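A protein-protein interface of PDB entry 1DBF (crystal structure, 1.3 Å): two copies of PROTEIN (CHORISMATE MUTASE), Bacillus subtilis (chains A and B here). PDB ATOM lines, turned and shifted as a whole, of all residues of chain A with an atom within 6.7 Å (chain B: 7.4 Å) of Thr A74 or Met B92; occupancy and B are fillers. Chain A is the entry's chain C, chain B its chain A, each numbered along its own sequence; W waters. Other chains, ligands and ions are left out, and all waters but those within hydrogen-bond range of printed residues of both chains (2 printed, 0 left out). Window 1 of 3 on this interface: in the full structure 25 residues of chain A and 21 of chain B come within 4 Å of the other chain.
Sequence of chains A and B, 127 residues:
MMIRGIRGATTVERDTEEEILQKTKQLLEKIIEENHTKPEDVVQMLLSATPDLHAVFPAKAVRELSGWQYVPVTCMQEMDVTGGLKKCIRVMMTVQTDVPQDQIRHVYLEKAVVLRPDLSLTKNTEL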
ATOM      1  N   VAL A  43      -4.093 -24.666  17.349  1.00  0.00           N
ATOM      2  CA  VAL A  43      -4.610 -24.133  16.093  1.00  0.00           C
ATOM      3  C   VAL A  43      -3.461 -23.907  15.121  1.00  0.00           C
ATOM      4  O   VAL A  43      -3.415 -24.380  13.985  1.00  0.00           O
ATOM      5  CB  VAL A  43      -5.394 -22.866  16.386  1.00  0.00           C
ATOM      6  CG1 VAL A  43      -5.852 -22.212  15.097  1.00  0.00           C
ATOM      7  CG2 VAL A  43      -6.591 -23.204  17.292  1.00  0.00           C
ATOM      8  N   GLN A  44      -2.478 -23.178  15.658  1.00  0.00           N
ATOM      9  CA  GLN A  44      -1.321 -22.752  14.887  1.00  0.00           C
ATOM     10  C   GLN A  44      -0.339 -22.069  15.815  1.00  0.00           C
ATOM     11  O   GLN A  44      -0.683 -21.736  16.962  1.00  0.00           O
ATOM     12  CB  GLN A  44      -1.713 -21.729  13.786  1.00  0.00           C
ATOM     13  CG  GLN A  44      -2.231 -20.443  14.325  1.00  0.00           C
ATOM     14  CD  GLN A  44      -2.741 -19.416  13.333  1.00  0.00           C
ATOM     15  OE1 GLN A  44      -2.360 -18.220  13.354  1.00  0.00           O
ATOM     16  NE2 GLN A  44      -3.626 -19.964  12.526  1.00  0.00           N
ATOM     17  N   MET A  45       0.849 -21.818  15.242  1.00  0.00           N
ATOM     18  CA  MET A  45       1.850 -21.058  15.974  1.00  0.00           C
ATOM     19  C   MET A  45       2.544 -20.075  15.037  1.00  0.00           C
ATOM     20  O   MET A  45       2.746 -20.419  13.866  1.00  0.00           O
ATOM     21  CB  MET A  45       2.944 -21.929  16.590  1.00  0.00           C
ATOM     22  CG  MET A  45       2.352 -22.927  17.556  1.00  0.00           C
ATOM     23  SD  MET A  45       3.642 -24.048  18.140  1.00  0.00           S
ATOM     24  CE  MET A  45       4.957 -22.969  18.660  1.00  0.00           C
ATOM     25  N   LEU A  46       2.945 -18.969  15.659  1.00  0.00           N
ATOM     26  CA  LEU A  46       3.852 -18.018  15.004  1.00  0.00           C
ATOM     27  C   LEU A  46       5.118 -17.854  15.827  1.00  0.00           C
ATOM     28  O   LEU A  46       5.043 -17.745  17.056  1.00  0.00           O
ATOM     29  CB  LEU A  46       3.185 -16.632  14.846  1.00  0.00           C
ATOM     30  CG  LEU A  46       1.907 -16.629  14.015  1.00  0.00           C
ATOM     31  CD1 LEU A  46       1.267 -15.256  14.041  1.00  0.00           C
ATOM     32  CD2 LEU A  46       2.205 -17.070  12.566  1.00  0.00           C
ATOM     33  N   LEU A  47       6.294 -17.755  15.191  1.00  0.00           N
ATOM     34  CA  LEU A  47       7.487 -17.436  15.965  1.00  0.00           C
ATOM     35  C   LEU A  47       8.190 -16.281  15.273  1.00  0.00           C
ATOM     36  O   LEU A  47       8.391 -16.365  14.038  1.00  0.00           O
ATOM     37  CB  LEU A  47       8.478 -18.616  16.010  1.00  0.00           C
ATOM     38  CG  LEU A  47       8.084 -19.781  16.931  1.00  0.00           C
ATOM     39  CD1 LEU A  47       7.166 -20.683  16.150  1.00  0.00           C
ATOM     40  CD2 LEU A  47       9.239 -20.604  17.443  1.00  0.00           C
ATOM     41  N   SER A  48       8.540 -15.262  16.087  1.00  0.00           N
ATOM     42  CA  SER A  48       9.269 -14.157  15.453  1.00  0.00           C
ATOM     43  C   SER A  48      10.716 -14.195  15.962  1.00  0.00           C
ATOM     44  O   SER A  48      11.039 -14.704  17.063  1.00  0.00           O
ATOM     45  CB  SER A  48       8.694 -12.782  15.810  1.00  0.00           C
ATOM     46  OG  SER A  48       8.927 -12.496  17.187  1.00  0.00           O
ATOM     47  N   ALA A  59      11.009 -22.117  13.964  1.00  0.00           N
ATOM     48  CA  ALA A  59       9.912 -23.053  13.782  1.00  0.00           C
ATOM     49  C   ALA A  59      10.457 -24.479  13.571  1.00  0.00           C
ATOM     50  O   ALA A  59       9.697 -25.439  13.804  1.00  0.00           O
ATOM     51  CB  ALA A  59       9.051 -22.710  12.564  1.00  0.00           C
ATOM     52  N   ARG A  63       8.705 -28.219  14.432  1.00  0.00           N
ATOM     53  CA  ARG A  63       8.473 -29.269  13.452  1.00  0.00           C
ATOM     54  C   ARG A  63       9.179 -30.545  13.869  1.00  0.00           C
ATOM     55  O   ARG A  63       8.799 -31.657  13.466  1.00  0.00           O
ATOM     56  CB  ARG A  63       8.937 -28.807  12.072  1.00  0.00           C
ATOM     57  CG  ARG A  63       8.218 -27.548  11.611  1.00  0.00           C
ATOM     58  CD  ARG A  63       8.349 -27.307  10.100  1.00  0.00           C
ATOM     59  NE  ARG A  63       7.584 -26.092   9.804  1.00  0.00           N
ATOM     60  CZ  ARG A  63       8.068 -24.895   9.566  1.00  0.00           C
ATOM     61  NH1 ARG A  63       9.370 -24.632   9.564  1.00  0.00           N
ATOM     62  NH2 ARG A  63       7.188 -23.933   9.333  1.00  0.00           N
ATOM     63  N   VAL A  71       1.472 -29.602  13.609  1.00  0.00           N
ATOM     64  CA  VAL A  71       1.087 -28.258  14.096  1.00  0.00           C
ATOM     65  C   VAL A  71       1.510 -27.196  13.081  1.00  0.00           C
ATOM     66  O   VAL A  71       2.720 -27.037  12.893  1.00  0.00           O
ATOM     67  CB  VAL A  71       1.674 -27.945  15.475  1.00  0.00           C
ATOM     68  CG1 VAL A  71       1.366 -26.531  15.933  1.00  0.00           C
ATOM     69  CG2 VAL A  71       1.168 -28.951  16.503  1.00  0.00           C
ATOM     70  N   PRO A  72       0.588 -26.437  12.466  1.00  0.00           N
ATOM     71  CA  PRO A  72       1.038 -25.450  11.468  1.00  0.00           C
ATOM     72  C   PRO A  72       1.758 -24.294  12.156  1.00  0.00           C
ATOM     73  O   PRO A  72       1.225 -23.762  13.130  1.00  0.00           O
ATOM     74  CB  PRO A  72      -0.228 -25.027  10.765  1.00  0.00           C
ATOM     75  CG  PRO A  72      -1.317 -25.304  11.729  1.00  0.00           C
ATOM     76  CD  PRO A  72      -0.880 -26.395  12.655  1.00  0.00           C
ATOM     77  N   VAL A  73       2.898 -23.950  11.589  1.00  0.00           N
ATOM     78  CA  VAL A  73       3.726 -22.898  12.210  1.00  0.00           C
ATOM     79  C   VAL A  73       4.380 -22.105  11.108  1.00  0.00           C
ATOM     80  O   VAL A  73       4.685 -22.646  10.035  1.00  0.00           O
ATOM     81  CB  VAL A  73       4.714 -23.511  13.234  1.00  0.00           C
ATOM     82  CG1 VAL A  73       5.566 -24.565  12.508  1.00  0.00           C
ATOM     83  CG2 VAL A  73       5.540 -22.464  13.939  1.00  0.00           C
ATOM     84  N   THR A  74       4.669 -20.858  11.353  1.00  0.00           N
ATOM     85  CA  THR A  74       5.491 -20.068  10.408  1.00  0.00           C
ATOM     86  C   THR A  74       6.143 -18.937  11.226  1.00  0.00           C
ATOM     87  O   THR A  74       5.747 -18.659  12.366  1.00  0.00           O
ATOM     88  CB  THR A  74       4.718 -19.636   9.163  1.00  0.00           C
ATOM     89  OG1 THR A  74       5.607 -19.289   8.096  1.00  0.00           O
ATOM     90  CG2 THR A  74       3.846 -18.422   9.489  1.00  0.00           C
ATOM     91  N   CYS A  75       7.122 -18.303  10.556  1.00  0.00           N
ATOM     92  CA  CYS A  75       7.943 -17.322  11.247  1.00  0.00           C
ATOM     93  C   CYS A  75       7.780 -15.924  10.632  1.00  0.00           C
ATOM     94  O   CYS A  75       7.191 -15.720   9.568  1.00  0.00           O
ATOM     95  CB  CYS A  75       9.461 -17.690  11.216  1.00  0.00           C
ATOM     96  SG  CYS A  75       9.717 -19.324  11.997  1.00  0.00           S
ATOM     97  N   MET A  76       8.262 -14.948  11.396  1.00  0.00           N
ATOM     98  CA  MET A  76       8.324 -13.591  10.835  1.00  0.00           C
ATOM     99  C   MET A  76       9.418 -12.845  11.561  1.00  0.00           C
ATOM    100  O   MET A  76       9.884 -13.257  12.627  1.00  0.00           O
ATOM    101  CB  MET A  76       6.998 -12.838  10.878  1.00  0.00           C
ATOM    102  CG  MET A  76       6.583 -12.332  12.259  1.00  0.00           C
ATOM    103  SD  MET A  76       6.053 -13.770  13.213  1.00  0.00           S
ATOM    104  CE  MET A  76       4.740 -12.970  14.138  1.00  0.00           C
ATOM    105  N   ARG B   4      -8.291 -24.331  12.687  1.00  0.00           N
ATOM    106  CA  ARG B   4      -6.995 -24.912  12.337  1.00  0.00           C
ATOM    107  C   ARG B   4      -6.274 -23.990  11.359  1.00  0.00           C
ATOM    108  O   ARG B   4      -6.914 -23.377  10.489  1.00  0.00           O
ATOM    109  CB  ARG B   4      -7.197 -26.215  11.577  1.00  0.00           C
ATOM    110  CG  ARG B   4      -8.005 -27.331  12.197  1.00  0.00           C
ATOM    111  CD  ARG B   4      -7.071 -28.159  13.085  1.00  0.00           C
ATOM    112  NE  ARG B   4      -7.781 -29.073  13.966  1.00  0.00           N
ATOM    113  CZ  ARG B   4      -7.197 -29.422  15.120  1.00  0.00           C
ATOM    114  NH1 ARG B   4      -6.011 -28.989  15.424  1.00  0.00           N
ATOM    115  NH2 ARG B   4      -7.865 -30.238  15.902  1.00  0.00           N
ATOM    116  N   GLY B   5      -4.937 -23.963  11.502  1.00  0.00           N
ATOM    117  CA  GLY B   5      -4.138 -23.322  10.501  1.00  0.00           C
ATOM    118  C   GLY B   5      -3.869 -24.197   9.274  1.00  0.00           C
ATOM    119  O   GLY B   5      -3.674 -25.396   9.375  1.00  0.00           O
ATOM    120  N   ILE B   6      -3.874 -23.545   8.103  1.00  0.00           N
ATOM    121  CA  ILE B   6      -3.417 -24.170   6.870  1.00  0.00           C
ATOM    122  C   ILE B   6      -2.223 -23.358   6.391  1.00  0.00           C
ATOM    123  O   ILE B   6      -2.281 -22.133   6.204  1.00  0.00           O
ATOM    124  CB  ILE B   6      -4.541 -24.195   5.814  1.00  0.00           C
ATOM    125  CG1 ILE B   6      -5.914 -24.670   6.382  1.00  0.00           C
ATOM    126  CG2 ILE B   6      -4.111 -24.996   4.592  1.00  0.00           C
ATOM    127  CD1 ILE B   6      -6.976 -24.828   5.306  1.00  0.00           C
ATOM    128  N   ARG B   7      -1.141 -24.094   6.129  1.00  0.00           N
ATOM    129  CA  ARG B   7       0.100 -23.493   5.640  1.00  0.00           C
ATOM    130  C   ARG B   7       0.213 -23.706   4.132  1.00  0.00           C
ATOM    131  O   ARG B   7      -0.209 -24.715   3.542  1.00  0.00           O
ATOM    132  CB  ARG B   7       1.320 -24.109   6.304  1.00  0.00           C
ATOM    133  CG  ARG B   7       1.628 -23.543   7.681  1.00  0.00           C
ATOM    134  CD  ARG B   7       2.068 -22.074   7.750  1.00  0.00           C
ATOM    135  NE  ARG B   7       2.813 -21.774   6.538  1.00  0.00           N
ATOM    136  CZ  ARG B   7       4.047 -22.285   6.280  1.00  0.00           C
ATOM    137  NH1 ARG B   7       4.698 -23.039   7.168  1.00  0.00           N
ATOM    138  NH2 ARG B   7       4.608 -21.994   5.102  1.00  0.00           N
ATOM    139  N   GLY B   8       0.822 -22.675   3.476  1.00  0.00           N
ATOM    140  CA  GLY B   8       1.196 -22.794   2.068  1.00  0.00           C
ATOM    141  C   GLY B   8       2.496 -22.038   1.867  1.00  0.00           C
ATOM    142  O   GLY B   8       2.898 -21.213   2.710  1.00  0.00           O
ATOM    143  N   ILE B  31      -4.890 -24.399  -2.322  1.00  0.00           N
ATOM    144  CA  ILE B  31      -5.395 -24.610  -0.960  1.00  0.00           C
ATOM    145  C   ILE B  31      -6.930 -24.828  -0.974  1.00  0.00           C
ATOM    146  O   ILE B  31      -7.396 -25.743  -0.277  1.00  0.00           O
ATOM    147  CB  ILE B  31      -4.992 -23.447  -0.062  1.00  0.00           C
ATOM    148  CG1 ILE B  31      -3.494 -23.386   0.149  1.00  0.00           C
ATOM    149  CG2 ILE B  31      -5.741 -23.556   1.267  1.00  0.00           C
ATOM    150  CD1 ILE B  31      -2.964 -22.322   1.056  1.00  0.00           C
ATOM    151  N   VAL B  42     -13.133 -18.767   6.870  1.00  0.00           N
ATOM    152  CA  VAL B  42     -11.753 -18.343   7.167  1.00  0.00           C
ATOM    153  C   VAL B  42     -11.775 -17.296   8.270  1.00  0.00           C
ATOM    154  O   VAL B  42     -12.397 -16.217   8.112  1.00  0.00           O
ATOM    155  CB  VAL B  42     -11.096 -17.753   5.917  1.00  0.00           C
ATOM    156  CG1 VAL B  42      -9.697 -17.284   6.220  1.00  0.00           C
ATOM    157  CG2 VAL B  42     -11.142 -18.843   4.831  1.00  0.00           C
ATOM    158  N   GLN B  44      -9.077 -15.734   9.504  1.00  0.00           N
ATOM    159  CA  GLN B  44      -8.134 -14.667   9.072  1.00  0.00           C
ATOM    160  C   GLN B  44      -6.989 -15.302   8.294  1.00  0.00           C
ATOM    161  O   GLN B  44      -6.838 -16.536   8.332  1.00  0.00           O
ATOM    162  CB  GLN B  44      -7.541 -13.949  10.298  1.00  0.00           C
ATOM    163  CG  GLN B  44      -6.641 -14.869  11.136  1.00  0.00           C
ATOM    164  CD  GLN B  44      -6.117 -14.247  12.412  1.00  0.00           C
ATOM    165  OE1 GLN B  44      -4.942 -14.330  12.779  1.00  0.00           O
ATOM    166  NE2 GLN B  44      -7.026 -13.595  13.139  1.00  0.00           N
ATOM    167  N   MET B  45      -6.173 -14.465   7.649  1.00  0.00           N
ATOM    168  CA  MET B  45      -5.016 -14.962   6.928  1.00  0.00           C
ATOM    169  C   MET B  45      -3.812 -14.053   7.180  1.00  0.00           C
ATOM    170  O   MET B  45      -3.983 -12.834   7.294  1.00  0.00           O
ATOM    171  CB  MET B  45      -5.232 -15.028   5.414  1.00  0.00           C
ATOM    172  CG  MET B  45      -6.406 -15.920   5.052  1.00  0.00           C
ATOM    173  SD  MET B  45      -6.620 -15.971   3.255  1.00  0.00           S
ATOM    174  CE  MET B  45      -4.954 -15.933   2.647  1.00  0.00           C
ATOM    175  N   LEU B  46      -2.617 -14.662   7.175  1.00  0.00           N
ATOM    176  CA  LEU B  46      -1.363 -13.919   7.231  1.00  0.00           C
ATOM    177  C   LEU B  46      -0.556 -14.391   6.020  1.00  0.00           C
ATOM    178  O   LEU B  46      -0.553 -15.574   5.646  1.00  0.00           O
ATOM    179  CB  LEU B  46      -0.563 -14.228   8.483  1.00  0.00           C
ATOM    180  CG  LEU B  46      -1.248 -13.790   9.808  1.00  0.00           C
ATOM    181  CD1 LEU B  46      -0.369 -14.218  10.996  1.00  0.00           C
ATOM    182  CD2 LEU B  46      -1.495 -12.297   9.842  1.00  0.00           C
ATOM    183  N   LEU B  47       0.080 -13.433   5.345  1.00  0.00           N
ATOM    184  CA  LEU B  47       1.002 -13.782   4.260  1.00  0.00           C
ATOM    185  C   LEU B  47       2.350 -13.169   4.555  1.00  0.00           C
ATOM    186  O   LEU B  47       2.373 -11.970   4.933  1.00  0.00           O
ATOM    187  CB  LEU B  47       0.472 -13.184   2.951  1.00  0.00           C
ATOM    188  CG  LEU B  47      -0.684 -13.917   2.301  1.00  0.00           C
ATOM    189  CD1 LEU B  47      -1.533 -13.018   1.421  1.00  0.00           C
ATOM    190  CD2 LEU B  47      -0.105 -15.011   1.396  1.00  0.00           C
ATOM    191  N   SER B  48       3.411 -13.929   4.389  1.00  0.00           N
ATOM    192  CA  SER B  48       4.767 -13.407   4.589  1.00  0.00           C
ATOM    193  C   SER B  48       5.521 -13.435   3.245  1.00  0.00           C
ATOM    194  O   SER B  48       5.208 -14.206   2.331  1.00  0.00           O
ATOM    195  CB  SER B  48       5.561 -14.152   5.652  1.00  0.00           C
ATOM    196  OG  SER B  48       6.049 -15.338   5.099  1.00  0.00           O
ATOM    197  N   PRO B  72     -10.306 -11.266   6.387  1.00  0.00           N
ATOM    198  CA  PRO B  72      -9.267 -10.351   6.917  1.00  0.00           C
ATOM    199  C   PRO B  72      -7.872 -10.958   6.707  1.00  0.00           C
ATOM    200  O   PRO B  72      -7.658 -12.129   7.005  1.00  0.00           O
ATOM    201  CB  PRO B  72      -9.584 -10.183   8.403  1.00  0.00           C
ATOM    202  CG  PRO B  72     -10.365 -11.413   8.724  1.00  0.00           C
ATOM    203  CD  PRO B  72     -11.017 -11.975   7.476  1.00  0.00           C
ATOM    204  N   VAL B  73      -7.018 -10.118   6.144  1.00  0.00           N
ATOM    205  CA  VAL B  73      -5.674 -10.587   5.802  1.00  0.00           C
ATOM    206  C   VAL B  73      -4.699  -9.424   6.008  1.00  0.00           C
ATOM    207  O   VAL B  73      -5.020  -8.225   5.856  1.00  0.00           O
ATOM    208  CB  VAL B  73      -5.667 -11.098   4.359  1.00  0.00           C
ATOM    209  CG1 VAL B  73      -6.046  -9.997   3.356  1.00  0.00           C
ATOM    210  CG2 VAL B  73      -4.311 -11.701   3.973  1.00  0.00           C
ATOM    211  N   THR B  74      -3.465  -9.790   6.393  1.00  0.00           N
ATOM    212  CA  THR B  74      -2.389  -8.810   6.462  1.00  0.00           C
ATOM    213  C   THR B  74      -1.058  -9.514   6.248  1.00  0.00           C
ATOM    214  O   THR B  74      -1.040 -10.750   6.301  1.00  0.00           O
ATOM    215  CB  THR B  74      -2.486  -8.004   7.779  1.00  0.00           C
ATOM    216  OG1 THR B  74      -1.751  -6.767   7.592  1.00  0.00           O
ATOM    217  CG2 THR B  74      -1.850  -8.681   8.949  1.00  0.00           C
ATOM    218  N   MET B  76       3.446  -9.704   6.431  1.00  0.00           N
ATOM    219  CA  MET B  76       4.602  -9.519   7.306  1.00  0.00           C
ATOM    220  C   MET B  76       5.864  -9.919   6.549  1.00  0.00           C
ATOM    221  O   MET B  76       5.797 -10.699   5.587  1.00  0.00           O
ATOM    222  CB  MET B  76       4.417 -10.423   8.550  1.00  0.00           C
ATOM    223  CG  MET B  76       4.138 -11.898   8.278  1.00  0.00           C
ATOM    224  SD  MET B  76       3.452 -12.773   9.683  1.00  0.00           S
ATOM    225  CE  MET B  76       3.633 -14.443   8.972  1.00  0.00           C
ATOM    226  N   GLU B  78       9.093 -12.058   6.249  1.00  0.00           N
ATOM    227  CA  GLU B  78       9.661 -13.343   6.714  1.00  0.00           C
ATOM    228  C   GLU B  78      11.074 -13.035   7.201  1.00  0.00           C
ATOM    229  O   GLU B  78      11.717 -12.072   6.717  1.00  0.00           O
ATOM    230  CB  GLU B  78       9.581 -14.411   5.617  1.00  0.00           C
ATOM    231  CG  GLU B  78      10.414 -15.673   5.856  1.00  0.00           C
ATOM    232  CD  GLU B  78       9.896 -16.596   6.963  1.00  0.00           C
ATOM    233  OE1 GLU B  78      10.006 -16.111   8.124  1.00  0.00           O
ATOM    234  OE2 GLU B  78       9.447 -17.749   6.698  1.00  0.00           O
ATOM    235  N   ARG B  90       4.808 -17.069   1.825  1.00  0.00           N
ATOM    236  CA  ARG B  90       4.179 -18.084   2.679  1.00  0.00           C
ATOM    237  C   ARG B  90       2.807 -17.596   3.163  1.00  0.00           C
ATOM    238  O   ARG B  90       2.597 -16.380   3.312  1.00  0.00           O
ATOM    239  CB  ARG B  90       5.066 -18.380   3.916  1.00  0.00           C
ATOM    240  CG  ARG B  90       6.392 -19.052   3.486  1.00  0.00           C
ATOM    241  CD  ARG B  90       7.334 -19.051   4.679  1.00  0.00           C
ATOM    242  NE  ARG B  90       8.555 -19.837   4.606  1.00  0.00           N
ATOM    243  CZ  ARG B  90       9.713 -19.402   4.085  1.00  0.00           C
ATOM    244  NH1 ARG B  90       9.808 -18.187   3.510  1.00  0.00           N
ATOM    245  NH2 ARG B  90      10.782 -20.171   4.098  1.00  0.00           N
ATOM    246  N   VAL B  91       1.935 -18.588   3.403  1.00  0.00           N
ATOM    247  CA  VAL B  91       0.617 -18.253   3.949  1.00  0.00           C
ATOM    248  C   VAL B  91       0.340 -19.068   5.215  1.00  0.00           C
ATOM    249  O   VAL B  91       0.725 -20.199   5.369  1.00  0.00           O
ATOM    250  CB  VAL B  91      -0.496 -18.481   2.921  1.00  0.00           C
ATOM    251  CG1 VAL B  91      -0.563 -19.914   2.429  1.00  0.00           C
ATOM    252  CG2 VAL B  91      -1.851 -18.089   3.517  1.00  0.00           C
ATOM    253  N   MET B  92      -0.378 -18.426   6.116  1.00  0.00           N
ATOM    254  CA  MET B  92      -1.006 -19.075   7.263  1.00  0.00           C
ATOM    255  C   MET B  92      -2.492 -18.678   7.245  1.00  0.00           C
ATOM    256  O   MET B  92      -2.856 -17.548   7.590  1.00  0.00           O
ATOM    257  CB  MET B  92      -0.484 -18.612   8.619  1.00  0.00           C
ATOM    258  CG  MET B  92      -1.186 -19.355   9.745  1.00  0.00           C
ATOM    259  SD  MET B  92      -0.726 -21.063  10.026  1.00  0.00           S
ATOM    260  CE  MET B  92       0.803 -20.911  10.907  1.00  0.00           C
ATOM    261  N   MET B  93      -3.361 -19.609   6.812  1.00  0.00           N
ATOM    262  CA  MET B  93      -4.797 -19.372   6.722  1.00  0.00           C
ATOM    263  C   MET B  93      -5.487 -20.068   7.886  1.00  0.00           C
ATOM    264  O   MET B  93      -5.353 -21.281   7.947  1.00  0.00           O
ATOM    265  CB  MET B  93      -5.377 -19.909   5.406  1.00  0.00           C
ATOM    266  CG  MET B  93      -6.891 -19.963   5.201  1.00  0.00           C
ATOM    267  SD  MET B  93      -7.434 -20.541   3.548  1.00  0.00           S
ATOM    268  CE  MET B  93      -5.915 -20.131   2.686  1.00  0.00           C
ATOM    269  N   THR B  94      -6.211 -19.282   8.706  1.00  0.00           N
ATOM    270  CA  THR B  94      -6.827 -19.844   9.907  1.00  0.00           C
ATOM    271  C   THR B  94      -8.290 -20.101   9.598  1.00  0.00           C
ATOM    272  O   THR B  94      -8.978 -19.125   9.201  1.00  0.00           O
ATOM    273  CB  THR B  94      -6.675 -18.816  11.048  1.00  0.00           C
ATOM    274  OG1 THR B  94      -5.316 -18.459  11.221  1.00  0.00           O
ATOM    275  CG2 THR B  94      -7.194 -19.464  12.333  1.00  0.00           C
ATOM    276  N   VAL B  95      -8.737 -21.363   9.755  1.00  0.00           N
ATOM    277  CA  VAL B  95     -10.091 -21.707   9.302  1.00  0.00           C
ATOM    278  C   VAL B  95     -10.860 -22.504  10.346  1.00  0.00           C
ATOM    279  O   VAL B  95     -10.301 -23.164  11.181  1.00  0.00           O
ATOM    280  CB  VAL B  95     -10.083 -22.591   8.027  1.00  0.00           C
ATOM    281  CG1 VAL B  95      -9.205 -21.897   6.989  1.00  0.00           C
ATOM    282  CG2 VAL B  95      -9.612 -24.000   8.329  1.00  0.00           C
ATOM    283  N   HIS B 106      -1.546 -28.933   3.582  1.00  0.00           N
ATOM    284  CA  HIS B 106      -0.653 -27.810   3.415  1.00  0.00           C
ATOM    285  C   HIS B 106      -0.063 -27.879   2.027  1.00  0.00           C
ATOM    286  O   HIS B 106       0.246 -28.997   1.541  1.00  0.00           O
ATOM    287  CB  HIS B 106       0.421 -27.915   4.489  1.00  0.00           C
ATOM    288  CG  HIS B 106      -0.231 -28.020   5.848  1.00  0.00           C
ATOM    289  ND1 HIS B 106      -0.319 -29.088   6.709  1.00  0.00           N
ATOM    290  CD2 HIS B 106      -0.914 -27.005   6.453  1.00  0.00           C
ATOM    291  CE1 HIS B 106      -0.995 -28.692   7.795  1.00  0.00           C
ATOM    292  NE2 HIS B 106      -1.370 -27.431   7.641  1.00  0.00           N
HETATM  293  O   HOH W   1      -4.076 -27.451  13.909  1.00  0.00           O
HETATM  294  O   HOH W   2       6.205 -16.803   7.326  1.00  0.00           O
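Leu A46 touches its own counterpart, Leu B46.
Met B76 touches its own counterpart, Met A76.
9 positions are printed for both chains.
Of the 20 pairs that touch across the chains among the printed residues, 2 have their exchanged pair printed and touching as well.
N of Gly B5 is in hydrogen-bond range of O of Val A43 (2.9 Å).
The backbone carbonyl oxygen of Val A73 is in hydrogen-bond range of the guanidinium group of Arg B7 (2.9 Å).
The side-chain hydroxyl of Thr B94 sits at hydrogen-bond distance from the side-chain amide nitrogen of Gln A44, at 2.6 Å.
The guanidinium group of Arg A63 lies close to the guanidinium group of Arg B7 (3.4 Å).
The backbone carbonyl oxygen (O) of Cys A75 sits close to the side-chain carboxylate (OE1) of Glu B78 (3.2 Å).
Water W2 lies within hydrogen-bond range of the side-chain hydroxyl of Thr A74 (2.7 Å), the side-chain hydroxyl of Ser B48 (2.7 Å), the backbone carbonyl oxygen of Cys A75 (2.7 Å) and the side-chain carboxylate of Glu B78 (3.4 Å).
Water W1 bridges NH1 of Arg B4 (2.9 Å) and O of Val A43 (3.1 Å).
O of Val B95 is in hydrogen-bond range of N of Arg B4 (2.8 Å).
The backbone carbonyl oxygen (O) of Arg B90 is in hydrogen-bond range of the backbone NH (N) of Ser B48, at 2.8 Å.
The backbone carbonyl oxygen (O) of Thr A74 lies within hydrogen-bond range of the backbone NH (N) of Leu A47.
The backbone carbonyl oxygen (O) of Leu A47 is in hydrogen-bond range of the backbone NH (N) of Met A76, at 3.0 Å.
N of Ala A59 lies close to SG of Cys A75 (3.7 Å).
The guanidinium group (NH2) of Arg A63 lies within hydrogen-bond range of the backbone carbonyl oxygen (O) of Val A73.
Hydrophobic or aromatic side chains of chain A that line the printed part of chain B: Leu A46, Pro A72 and Met A76.
Among the printed residues, 20 pairs touch across the chains.
Gln A44 touches Gly B5 (NE2 to CA, 3.95 Å).
O of Met A45 touches CE of Met B92 (3.6 Å).
Leu A46 touches Leu B46 (CD1 to CD1, 3.6 Å).
CG of Pro A72 touches O of Gly B5, 3.3 Å away.
Pro A72 touches Met B92 (O to CE, 3.6 Å).
N of Val A73 touches CE of Met B92, 3.8 Å away.
Thr A74 touches Arg B90 (OG1 to CD, 3.8 Å).
N of Thr A74 touches CE of Met B92 (3.9 Å).
O of Cys A75 touches CE of Met B76 (3.8 Å).
Glu B78 touches Met A76 (OE1 to N, 3.9 Å).
Printed residues of chain B within 4 Å of Val A43: Arg B4 and Gly B5.
Printed residues of chain B within 4 Å of Gln A44: Gly B5 (3.95 Å), Met B92 (3.7 Å) and Thr B94 (2.6 Å).
Leu A47 touches none of the printed residues of chain B.
Of the printed residues of chain B, Thr A74 touches Arg B7, Arg B90 and Met B92.
Of the printed residues of chain A, Arg B4 touches Val A43.
Of the printed residues of chain A, Glu B78 touches Cys A75 (3.2 Å) and Met A76 (3.9 Å).
Printed residues of chain A within 4 Å of Met B92: Gln A44, Met A45, Pro A72, Val A73 and Thr A74.
The nearest printed residue of chain B that does not touch Thr A74 is Met B76 (4.02 Å).
The nearest printed residue of chain B that does not touch Gln A44 is Gln B44 (4.7 Å).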
